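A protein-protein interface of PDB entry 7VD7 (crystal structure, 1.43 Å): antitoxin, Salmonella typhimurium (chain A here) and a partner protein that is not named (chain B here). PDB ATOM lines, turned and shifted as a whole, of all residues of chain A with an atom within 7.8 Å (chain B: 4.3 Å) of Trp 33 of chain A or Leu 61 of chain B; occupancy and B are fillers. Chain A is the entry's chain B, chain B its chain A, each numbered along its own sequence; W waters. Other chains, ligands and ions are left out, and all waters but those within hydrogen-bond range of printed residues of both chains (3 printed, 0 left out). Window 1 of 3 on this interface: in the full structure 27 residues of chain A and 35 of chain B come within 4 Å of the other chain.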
ATOM      1  N   TYR A  22      -7.803 -23.033  10.236  1.00  0.00           N
ATOM      2  CA  TYR A  22      -6.937 -23.339   9.079  1.00  0.00           C
ATOM      3  C   TYR A  22      -5.479 -23.674   9.440  1.00  0.00           C
ATOM      4  O   TYR A  22      -4.646 -23.737   8.531  1.00  0.00           O
ATOM      5  CB  TYR A  22      -6.937 -22.122   8.159  1.00  0.00           C
ATOM      6  CG  TYR A  22      -8.265 -21.782   7.558  1.00  0.00           C
ATOM      7  CD1 TYR A  22      -8.773 -22.557   6.535  1.00  0.00           C
ATOM      8  CD2 TYR A  22      -9.019 -20.704   7.965  1.00  0.00           C
ATOM      9  CE1 TYR A  22      -9.969 -22.276   5.931  1.00  0.00           C
ATOM     10  CE2 TYR A  22     -10.242 -20.418   7.390  1.00  0.00           C
ATOM     11  CZ  TYR A  22     -10.719 -21.195   6.343  1.00  0.00           C
ATOM     12  OH  TYR A  22     -11.904 -20.914   5.725  1.00  0.00           O
ATOM     13  N   ILE A  25      -4.764 -27.319   7.744  1.00  0.00           N
ATOM     14  CA  ILE A  25      -5.064 -27.334   6.297  1.00  0.00           C
ATOM     15  C   ILE A  25      -5.435 -25.912   5.925  1.00  0.00           C
ATOM     16  O   ILE A  25      -6.547 -25.464   6.148  1.00  0.00           O
ATOM     17  CB  ILE A  25      -6.182 -28.352   5.928  1.00  0.00           C
ATOM     18  CG1 ILE A  25      -5.906 -29.768   6.405  1.00  0.00           C
ATOM     19  CG2 ILE A  25      -6.343 -28.347   4.418  1.00  0.00           C
ATOM     20  CD1 ILE A  25      -7.066 -30.734   6.164  1.00  0.00           C
ATOM     21  N   PRO A  26      -4.475 -25.168   5.335  1.00  0.00           N
ATOM     22  CA  PRO A  26      -4.749 -23.773   5.011  1.00  0.00           C
ATOM     23  C   PRO A  26      -5.924 -23.557   4.052  1.00  0.00           C
ATOM     24  O   PRO A  26      -6.258 -24.482   3.273  1.00  0.00           O
ATOM     25  CB  PRO A  26      -3.460 -23.295   4.324  1.00  0.00           C
ATOM     26  CG  PRO A  26      -2.389 -24.251   4.798  1.00  0.00           C
ATOM     27  CD  PRO A  26      -3.095 -25.570   5.073  1.00  0.00           C
ATOM     28  N   ALA A  27      -6.457 -22.344   4.009  1.00  0.00           N
ATOM     29  CA  ALA A  27      -7.466 -21.888   3.030  1.00  0.00           C
ATOM     30  C   ALA A  27      -6.851 -21.967   1.635  1.00  0.00           C
ATOM     31  O   ALA A  27      -5.618 -21.821   1.485  1.00  0.00           O
ATOM     32  CB  ALA A  27      -7.944 -20.488   3.351  1.00  0.00           C
ATOM     33  N   SER A  28      -7.704 -22.236   0.645  1.00  0.00           N
ATOM     34  CA  SER A  28      -7.332 -22.434  -0.779  1.00  0.00           C
ATOM     35  C   SER A  28      -7.933 -21.310  -1.627  1.00  0.00           C
ATOM     36  O   SER A  28      -8.738 -20.517  -1.106  1.00  0.00           O
ATOM     37  CB  SER A  28      -7.804 -23.790  -1.274  1.00  0.00           C
ATOM     38  OG  SER A  28      -9.050 -24.139  -0.685  1.00  0.00           O
ATOM     39  N   GLU A  29      -7.610 -21.326  -2.923  1.00  0.00           N
ATOM     40  CA  GLU A  29      -8.267 -20.422  -3.895  1.00  0.00           C
ATOM     41  C   GLU A  29      -8.738 -21.320  -5.047  1.00  0.00           C
ATOM     42  O   GLU A  29      -8.139 -22.376  -5.245  1.00  0.00           O
ATOM     43  CB  GLU A  29      -7.331 -19.331  -4.448  1.00  0.00           C
ATOM     44  CG  GLU A  29      -7.534 -17.964  -3.838  1.00  0.00           C
ATOM     45  CD  GLU A  29      -6.560 -16.941  -4.393  1.00  0.00           C
ATOM     46  OE1 GLU A  29      -6.391 -15.886  -3.765  1.00  0.00           O
ATOM     47  OE2 GLU A  29      -5.960 -17.218  -5.448  1.00  0.00           O
ATOM     48  N   ASP A  30      -9.739 -20.877  -5.800  1.00  0.00           N
ATOM     49  CA  ASP A  30     -10.276 -21.606  -6.982  1.00  0.00           C
ATOM     50  C   ASP A  30      -9.131 -22.106  -7.887  1.00  0.00           C
ATOM     51  O   ASP A  30      -9.232 -23.235  -8.400  1.00  0.00           O
ATOM     52  CB  ASP A  30     -11.266 -20.722  -7.740  1.00  0.00           C
ATOM     53  CG  ASP A  30     -12.415 -21.507  -8.335  1.00  0.00           C
ATOM     54  OD1 ASP A  30     -12.140 -22.446  -9.113  1.00  0.00           O
ATOM     55  OD2 ASP A  30     -13.574 -21.200  -7.985  1.00  0.00           O
ATOM     56  N   GLY A  31      -8.076 -21.304  -8.077  1.00  0.00           N
ATOM     57  CA  GLY A  31      -6.924 -21.638  -8.944  1.00  0.00           C
ATOM     58  C   GLY A  31      -6.155 -22.863  -8.483  1.00  0.00           C
ATOM     59  O   GLY A  31      -5.757 -23.667  -9.346  1.00  0.00           O
ATOM     60  N   GLN A  32      -5.964 -23.035  -7.170  1.00  0.00           N
ATOM     61  CA  GLN A  32      -5.302 -24.247  -6.605  1.00  0.00           C
ATOM     62  C   GLN A  32      -6.129 -25.513  -6.916  1.00  0.00           C
ATOM     63  O   GLN A  32      -5.509 -26.593  -6.976  1.00  0.00           O
ATOM     64  CB  GLN A  32      -5.034 -24.090  -5.108  1.00  0.00           C
ATOM     65  CG  GLN A  32      -4.100 -22.931  -4.787  1.00  0.00           C
ATOM     66  CD  GLN A  32      -4.232 -22.490  -3.350  1.00  0.00           C
ATOM     67  OE1 GLN A  32      -4.467 -21.319  -3.047  1.00  0.00           O
ATOM     68  NE2 GLN A  32      -4.149 -23.451  -2.445  1.00  0.00           N
ATOM     69  N   TRP A  33      -7.446 -25.385  -7.165  1.00  0.00           N
ATOM     70  CA  TRP A  33      -8.368 -26.520  -7.494  1.00  0.00           C
ATOM     71  C   TRP A  33      -8.669 -26.613  -8.998  1.00  0.00           C
ATOM     72  O   TRP A  33      -9.726 -27.203  -9.355  1.00  0.00           O
ATOM     73  CB  TRP A  33      -9.671 -26.387  -6.709  1.00  0.00           C
ATOM     74  CG  TRP A  33      -9.465 -26.666  -5.250  1.00  0.00           C
ATOM     75  CD1 TRP A  33      -9.140 -25.742  -4.313  1.00  0.00           C
ATOM     76  CD2 TRP A  33      -9.573 -27.933  -4.565  1.00  0.00           C
ATOM     77  NE1 TRP A  33      -9.061 -26.328  -3.082  1.00  0.00           N
ATOM     78  CE2 TRP A  33      -9.294 -27.664  -3.213  1.00  0.00           C
ATOM     79  CE3 TRP A  33      -9.887 -29.246  -4.943  1.00  0.00           C
ATOM     80  CZ2 TRP A  33      -9.315 -28.648  -2.232  1.00  0.00           C
ATOM     81  CZ3 TRP A  33      -9.893 -30.231  -3.969  1.00  0.00           C
ATOM     82  CH2 TRP A  33      -9.622 -29.924  -2.641  1.00  0.00           C
ATOM     83  N   SER A  34      -7.781 -26.109  -9.858  1.00  0.00           N
ATOM     84  CA  SER A  34      -7.949 -26.168 -11.339  1.00  0.00           C
ATOM     85  C   SER A  34      -7.642 -27.586 -11.859  1.00  0.00           C
ATOM     86  O   SER A  34      -8.282 -27.986 -12.852  1.00  0.00           O
ATOM     87  CB  SER A  34      -7.087 -25.119 -12.042  1.00  0.00           C
ATOM     88  OG  SER A  34      -5.881 -25.715 -12.520  1.00  0.00           O
ATOM     89  N   GLU A  35      -6.661 -28.298 -11.288  1.00  0.00           N
ATOM     90  CA  GLU A  35      -6.194 -29.617 -11.792  1.00  0.00           C
ATOM     91  C   GLU A  35      -6.812 -30.759 -10.958  1.00  0.00           C
ATOM     92  O   GLU A  35      -6.370 -31.921 -11.102  1.00  0.00           O
ATOM     93  CB  GLU A  35      -4.663 -29.656 -11.811  1.00  0.00           C
ATOM     94  CG  GLU A  35      -4.054 -28.501 -12.611  1.00  0.00           C
ATOM     95  CD  GLU A  35      -2.636 -28.691 -13.131  1.00  0.00           C
ATOM     96  OE1 GLU A  35      -2.180 -29.854 -13.247  1.00  0.00           O
ATOM     97  OE2 GLU A  35      -1.984 -27.661 -13.440  1.00  0.00           O
ATOM     98  N   ALA A  36      -7.862 -30.484 -10.189  1.00  0.00           N
ATOM     99  CA  ALA A  36      -8.481 -31.539  -9.349  1.00  0.00           C
ATOM    100  C   ALA A  36      -9.126 -32.614 -10.234  1.00  0.00           C
ATOM    101  O   ALA A  36      -9.518 -32.346 -11.386  1.00  0.00           O
ATOM    102  CB  ALA A  36      -9.462 -30.954  -8.367  1.00  0.00           C
ATOM    103  N   VAL A  37      -9.292 -33.796  -9.666  1.00  0.00           N
ATOM    104  CA  VAL A  37     -10.005 -34.948 -10.298  1.00  0.00           C
ATOM    105  C   VAL A  37     -11.236 -35.250  -9.423  1.00  0.00           C
ATOM    106  O   VAL A  37     -11.107 -35.386  -8.173  1.00  0.00           O
ATOM    107  CB  VAL A  37      -9.078 -36.157 -10.477  1.00  0.00           C
ATOM    108  CG1 VAL A  37      -9.832 -37.364 -11.013  1.00  0.00           C
ATOM    109  CG2 VAL A  37      -7.900 -35.829 -11.391  1.00  0.00           C
ATOM    110  N   LEU B  35     -13.878 -34.593  -4.600  1.00  0.00           N
ATOM    111  CA  LEU B  35     -13.033 -33.790  -5.516  1.00  0.00           C
ATOM    112  C   LEU B  35     -11.635 -33.732  -4.928  1.00  0.00           C
ATOM    113  O   LEU B  35     -11.517 -33.298  -3.757  1.00  0.00           O
ATOM    114  CB  LEU B  35     -13.629 -32.400  -5.635  1.00  0.00           C
ATOM    115  CG  LEU B  35     -12.909 -31.504  -6.644  1.00  0.00           C
ATOM    116  CD1 LEU B  35     -13.147 -31.990  -8.086  1.00  0.00           C
ATOM    117  CD2 LEU B  35     -13.341 -30.048  -6.521  1.00  0.00           C
ATOM    118  N   SER B  36     -10.619 -34.132  -5.655  1.00  0.00           N
ATOM    119  CA  SER B  36      -9.258 -34.397  -5.115  1.00  0.00           C
ATOM    120  C   SER B  36      -8.244 -33.559  -5.882  1.00  0.00           C
ATOM    121  O   SER B  36      -8.325 -33.561  -7.112  1.00  0.00           O
ATOM    122  CB  SER B  36      -8.842 -35.828  -5.175  1.00  0.00           C
ATOM    123  OG  SER B  36      -9.771 -36.685  -4.491  1.00  0.00           O
ATOM    124  N   ARG B  37      -7.292 -32.956  -5.186  1.00  0.00           N
ATOM    125  CA  ARG B  37      -6.113 -32.264  -5.809  1.00  0.00           C
ATOM    126  C   ARG B  37      -4.801 -32.778  -5.230  1.00  0.00           C
ATOM    127  O   ARG B  37      -4.718 -33.059  -4.038  1.00  0.00           O
ATOM    128  CB  ARG B  37      -6.201 -30.755  -5.676  1.00  0.00           C
ATOM    129  CG  ARG B  37      -5.891 -30.178  -4.301  1.00  0.00           C
ATOM    130  CD  ARG B  37      -5.991 -28.668  -4.363  1.00  0.00           C
ATOM    131  NE  ARG B  37      -5.616 -28.056  -3.115  1.00  0.00           N
ATOM    132  CZ  ARG B  37      -4.374 -27.707  -2.802  1.00  0.00           C
ATOM    133  NH1 ARG B  37      -3.401 -27.894  -3.672  1.00  0.00           N
ATOM    134  NH2 ARG B  37      -4.114 -27.167  -1.624  1.00  0.00           N
ATOM    135  N   GLN B  49      -5.404 -33.499  -1.282  1.00  0.00           N
ATOM    136  CA  GLN B  49      -6.540 -32.992  -0.489  1.00  0.00           C
ATOM    137  C   GLN B  49      -7.799 -33.402  -1.186  1.00  0.00           C
ATOM    138  O   GLN B  49      -7.909 -33.236  -2.394  1.00  0.00           O
ATOM    139  CB  GLN B  49      -6.477 -31.476  -0.329  1.00  0.00           C
ATOM    140  CG  GLN B  49      -5.283 -31.032   0.484  1.00  0.00           C
ATOM    141  CD  GLN B  49      -5.441 -29.588   0.855  1.00  0.00           C
ATOM    142  OE1 GLN B  49      -6.499 -29.002   0.675  1.00  0.00           O
ATOM    143  NE2 GLN B  49      -4.351 -28.976   1.285  1.00  0.00           N
ATOM    144  N   THR B  50      -8.793 -33.852  -0.455  1.00  0.00           N
ATOM    145  CA  THR B  50     -10.071 -34.333  -1.020  1.00  0.00           C
ATOM    146  C   THR B  50     -11.230 -33.705  -0.270  1.00  0.00           C
ATOM    147  O   THR B  50     -11.302 -33.815   0.982  1.00  0.00           O
ATOM    148  CB  THR B  50     -10.131 -35.863  -0.998  1.00  0.00           C
ATOM    149  OG1 THR B  50      -9.142 -36.425  -1.849  1.00  0.00           O
ATOM    150  CG2 THR B  50     -11.471 -36.442  -1.401  1.00  0.00           C
ATOM    151  N   LEU B  51     -12.210 -33.212  -1.033  1.00  0.00           N
ATOM    152  CA  LEU B  51     -13.500 -32.732  -0.515  1.00  0.00           C
ATOM    153  C   LEU B  51     -14.580 -33.785  -0.719  1.00  0.00           C
ATOM    154  O   LEU B  51     -14.679 -34.333  -1.819  1.00  0.00           O
ATOM    155  CB  LEU B  51     -13.923 -31.450  -1.242  1.00  0.00           C
ATOM    156  CG  LEU B  51     -13.033 -30.254  -0.952  1.00  0.00           C
ATOM    157  CD1 LEU B  51     -13.087 -29.300  -2.145  1.00  0.00           C
ATOM    158  CD2 LEU B  51     -13.477 -29.586   0.338  1.00  0.00           C
ATOM    159  N   ILE B  60     -16.571 -32.146   4.127  1.00  0.00           N
ATOM    160  CA  ILE B  60     -15.275 -32.056   4.818  1.00  0.00           C
ATOM    161  C   ILE B  60     -14.138 -32.059   3.820  1.00  0.00           C
ATOM    162  O   ILE B  60     -14.239 -32.602   2.735  1.00  0.00           O
ATOM    163  CB  ILE B  60     -15.186 -33.135   5.904  1.00  0.00           C
ATOM    164  CG1 ILE B  60     -15.174 -34.513   5.310  1.00  0.00           C
ATOM    165  CG2 ILE B  60     -16.228 -32.962   7.002  1.00  0.00           C
ATOM    166  CD1 ILE B  60     -14.648 -35.531   6.300  1.00  0.00           C
ATOM    167  N   LEU B  61     -13.055 -31.410   4.222  1.00  0.00           N
ATOM    168  CA  LEU B  61     -11.763 -31.398   3.518  1.00  0.00           C
ATOM    169  C   LEU B  61     -10.794 -32.311   4.246  1.00  0.00           C
ATOM    170  O   LEU B  61     -10.542 -32.115   5.444  1.00  0.00           O
ATOM    171  CB  LEU B  61     -11.266 -29.957   3.432  1.00  0.00           C
ATOM    172  CG  LEU B  61      -9.903 -29.793   2.756  1.00  0.00           C
ATOM    173  CD1 LEU B  61      -9.881 -30.226   1.309  1.00  0.00           C
ATOM    174  CD2 LEU B  61      -9.503 -28.341   2.821  1.00  0.00           C
ATOM    175  N   VAL B  62     -10.194 -33.256   3.527  1.00  0.00           N
ATOM    176  CA  VAL B  62      -9.285 -34.271   4.085  1.00  0.00           C
ATOM    177  C   VAL B  62      -7.924 -34.156   3.458  1.00  0.00           C
ATOM    178  O   VAL B  62      -7.822 -34.230   2.224  1.00  0.00           O
ATOM    179  CB  VAL B  62      -9.859 -35.679   3.880  1.00  0.00           C
ATOM    180  CG1 VAL B  62      -8.903 -36.711   4.480  1.00  0.00           C
ATOM    181  CG2 VAL B  62     -11.260 -35.826   4.475  1.00  0.00           C
ATOM    182  N   ALA B  63      -6.906 -33.985   4.247  1.00  0.00           N
ATOM    183  CA  ALA B  63      -5.487 -34.021   3.825  1.00  0.00           C
ATOM    184  C   ALA B  63      -4.986 -35.433   4.029  1.00  0.00           C
ATOM    185  O   ALA B  63      -5.234 -36.017   5.120  1.00  0.00           O
ATOM    186  CB  ALA B  63      -4.652 -33.064   4.609  1.00  0.00           C
ATOM    187  N   SER B  79      -5.051 -35.052   8.215  1.00  0.00           N
ATOM    188  CA  SER B  79      -5.798 -33.959   8.881  1.00  0.00           C
ATOM    189  C   SER B  79      -7.167 -33.859   8.227  1.00  0.00           C
ATOM    190  O   SER B  79      -7.352 -34.271   7.071  1.00  0.00           O
ATOM    191  CB  SER B  79      -5.077 -32.639   8.751  1.00  0.00           C
ATOM    192  OG  SER B  79      -5.681 -31.629   9.514  1.00  0.00           O
ATOM    193  N   ALA B  80      -8.125 -33.263   8.890  1.00  0.00           N
ATOM    194  CA  ALA B  80      -9.453 -33.073   8.271  1.00  0.00           C
ATOM    195  C   ALA B  80     -10.174 -31.946   8.960  1.00  0.00           C
ATOM    196  O   ALA B  80     -10.036 -31.795  10.191  1.00  0.00           O
ATOM    197  CB  ALA B  80     -10.282 -34.345   8.318  1.00  0.00           C
ATOM    198  N   ARG B  81     -10.914 -31.150   8.205  1.00  0.00           N
ATOM    199  CA  ARG B  81     -11.721 -30.084   8.832  1.00  0.00           C
ATOM    200  C   ARG B  81     -12.950 -29.817   7.979  1.00  0.00           C
ATOM    201  O   ARG B  81     -13.024 -30.309   6.868  1.00  0.00           O
ATOM    202  CB  ARG B  81     -10.918 -28.785   8.987  1.00  0.00           C
ATOM    203  CG  ARG B  81     -10.284 -28.271   7.703  1.00  0.00           C
ATOM    204  CD  ARG B  81      -9.976 -26.786   7.803  1.00  0.00           C
ATOM    205  NE  ARG B  81      -9.266 -26.267   6.648  1.00  0.00           N
ATOM    206  CZ  ARG B  81      -9.840 -25.854   5.529  1.00  0.00           C
ATOM    207  NH1 ARG B  81     -11.155 -25.878   5.405  1.00  0.00           N
ATOM    208  NH2 ARG B  81      -9.092 -25.404   4.541  1.00  0.00           N
ATOM    209  N   ALA B  83     -15.134 -28.044   5.350  1.00  0.00           N
ATOM    210  CA  ALA B  83     -14.894 -27.200   4.172  1.00  0.00           C
ATOM    211  C   ALA B  83     -15.488 -25.794   4.409  1.00  0.00           C
ATOM    212  O   ALA B  83     -16.634 -25.690   4.933  1.00  0.00           O
ATOM    213  CB  ALA B  83     -15.492 -27.880   2.936  1.00  0.00           C
ATOM    214  N   GLU B  87     -14.490 -23.762  -0.768  1.00  0.00           N
ATOM    215  CA  GLU B  87     -14.234 -25.214  -0.963  1.00  0.00           C
ATOM    216  C   GLU B  87     -15.576 -25.911  -1.227  1.00  0.00           C
ATOM    217  O   GLU B  87     -15.684 -26.763  -2.114  1.00  0.00           O
ATOM    218  CB  GLU B  87     -13.515 -25.760   0.281  1.00  0.00           C
ATOM    219  CG  GLU B  87     -12.069 -25.383   0.385  1.00  0.00           C
ATOM    220  CD  GLU B  87     -11.519 -25.340   1.813  1.00  0.00           C
ATOM    221  OE1 GLU B  87     -12.290 -25.717   2.732  1.00  0.00           O
ATOM    222  OE2 GLU B  87     -10.325 -25.005   1.909  1.00  0.00           O
ATOM    223  N   ARG B  90     -16.405 -25.299  -4.945  1.00  0.00           N
ATOM    224  CA  ARG B  90     -15.654 -26.202  -5.857  1.00  0.00           C
ATOM    225  C   ARG B  90     -16.282 -27.618  -5.779  1.00  0.00           C
ATOM    226  O   ARG B  90     -16.475 -28.247  -6.834  1.00  0.00           O
ATOM    227  CB  ARG B  90     -14.163 -26.273  -5.486  1.00  0.00           C
ATOM    228  CG  ARG B  90     -13.412 -24.946  -5.493  1.00  0.00           C
ATOM    229  CD  ARG B  90     -13.536 -24.181  -6.792  1.00  0.00           C
ATOM    230  NE  ARG B  90     -13.380 -25.040  -7.955  1.00  0.00           N
ATOM    231  CZ  ARG B  90     -14.032 -24.904  -9.117  1.00  0.00           C
ATOM    232  NH1 ARG B  90     -14.886 -23.910  -9.303  1.00  0.00           N
ATOM    233  NH2 ARG B  90     -13.811 -25.769 -10.097  1.00  0.00           N
HETATM  234  O   HOH W   1      -4.486 -25.941   1.639  1.00  0.00           O
HETATM  235  O   HOH W   2     -10.459 -22.308   1.203  1.00  0.00           O
HETATM  236  O   HOH W   3      -6.837 -26.684  -0.561  1.00  0.00           O
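The backbone carbonyl oxygen (O) of Ser 36 of chain B lies within hydrogen-bond range of the backbone NH (N) of Val 37 of chain A.
The backbone carbonyl oxygen of Ile 25 of chain A is in hydrogen-bond range of the guanidinium group of Arg 81 of chain B, 2.9 Å away.
The backbone carbonyl oxygen of Pro 26 of chain A lies within hydrogen-bond range of the guanidinium group of Arg 81 of chain B (3.2 Å).
OG of Ser 28 of chain A is in hydrogen-bond range of OE2 of Glu 87 of chain B (3.0 Å).
NE of Arg 90 of chain B lies within salt-bridge range of OD1 of Asp 30 of chain A (3.1 Å).
The side-chain hydroxyl (OG) of Ser 36 of chain B is in hydrogen-bond range of the side-chain hydroxyl (OG1) of Thr 50 of chain B, at 2.7 Å.
N of Arg 37 of chain B is in hydrogen-bond range of O of Gln 49 of chain B (2.9 Å).
The backbone NH of Leu 61 of chain B is in hydrogen-bond range of the backbone carbonyl oxygen of Arg 81 of chain B, 2.9 Å away.
O of Ser 79 of chain B sits at hydrogen-bond distance from N of Ala 63 of chain B (2.9 Å).
NE1 of Trp 33 of chain A lies within hydrogen-bond range of OG of Ser 28 of chain A.
N of Glu 29 of chain A sits at hydrogen-bond distance from OE1 of Gln 32 of chain A, at 3.1 Å.
CG2 of Ile 25 of chain A touches NE2 of Gln 49 of chain B (3.8 Å).
Ala 63 of chain B touches Ile 25 of chain A.
Gln 32 of chain A touches Arg 37 of chain B (O to CD, 3.4 Å).
CZ3 of Trp 33 of chain A touches O of Leu 35 of chain B, at 3.5 Å.
Arg 37 of chain B touches Trp 33 of chain A.
Gln 49 of chain B touches Trp 33 of chain A (O to CH2, 3.7 Å).
CH2 of Trp 33 of chain A touches CD1 of Leu 51 of chain B (3.6 Å).
Trp 33 of chain A touches Leu 61 of chain B.
CB of Ala 36 of chain A touches CD1 of Leu 35 of chain B, 3.8 Å away.
Ala 36 of chain A touches Ser 36 of chain B.
Of chain B, only Leu 35 (3.5 Å), Arg 37 (3.6 Å), Gln 49 (3.7 Å), Leu 51 (3.6 Å) and Leu 61 (3.9 Å) come within 4 Å of Trp 33 of chain A.
Of chain A, only Ile 25 (3.5 Å) and Trp 33 (3.9 Å) come within 4 Å of Leu 61 of chain B.
Of the printed residues of chain A, Arg 90 of chain B touches Asp 30 (3.1 Å).
Of the printed residues of chain B, Ile 25 of chain A touches Gln 49, Leu 61, Ala 63, Ser 79, Ala 80 and Arg 81.
Printed residues of chain A within 4 Å of Leu 51 of chain B: Trp 33.
Of the printed residues of chain A, Leu 35 of chain B touches Trp 33, Ala 36 and Val 37.
Glu 29 of chain A touches none of the printed residues of chain B.
Ala 83 of chain B touches none of the printed residues of chain A.
The nearest printed residue of chain B that does not touch Val 37 of chain A is Arg 37 of chain B (5.0 Å).
Printed residues of chain A that touch a printed residue of chain B: Tyr 22, Ile 25, Pro 26, Ser 28, Asp 30, Gln 32, Trp 33, Ala 36 and Val 37.
Hydrophobic or aromatic side chains of chain A that line the printed part of chain B: Tyr 22, Ile 25, Trp 33 and Ala 36.
Of the 16 printed residues of chain B, 12 touch a printed residue of chain A.
Water W3 lies within hydrogen-bond range of the side-chain amide oxygen (OE1) of Gln 49 of chain B (2.6 Å), the guanidinium group (NH2) of Arg 37 of chain B (3.0 Å), the side-chain hydroxyl (OG) of Ser 28 of chain A (3.4 Å) and the indole nitrogen (NE1) of Trp 33 of chain A (3.4 Å).
Water W2 lies within hydrogen-bond range of OE2 of Glu 87 of chain B (2.8 Å) and N of Ser 28 of chain A (2.8 Å).
Water W1 lies within hydrogen-bond range of the backbone carbonyl oxygen of Pro 26 of chain A (2.8 Å) and the side-chain amide nitrogen of Gln 49 of chain B (3.1 Å).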
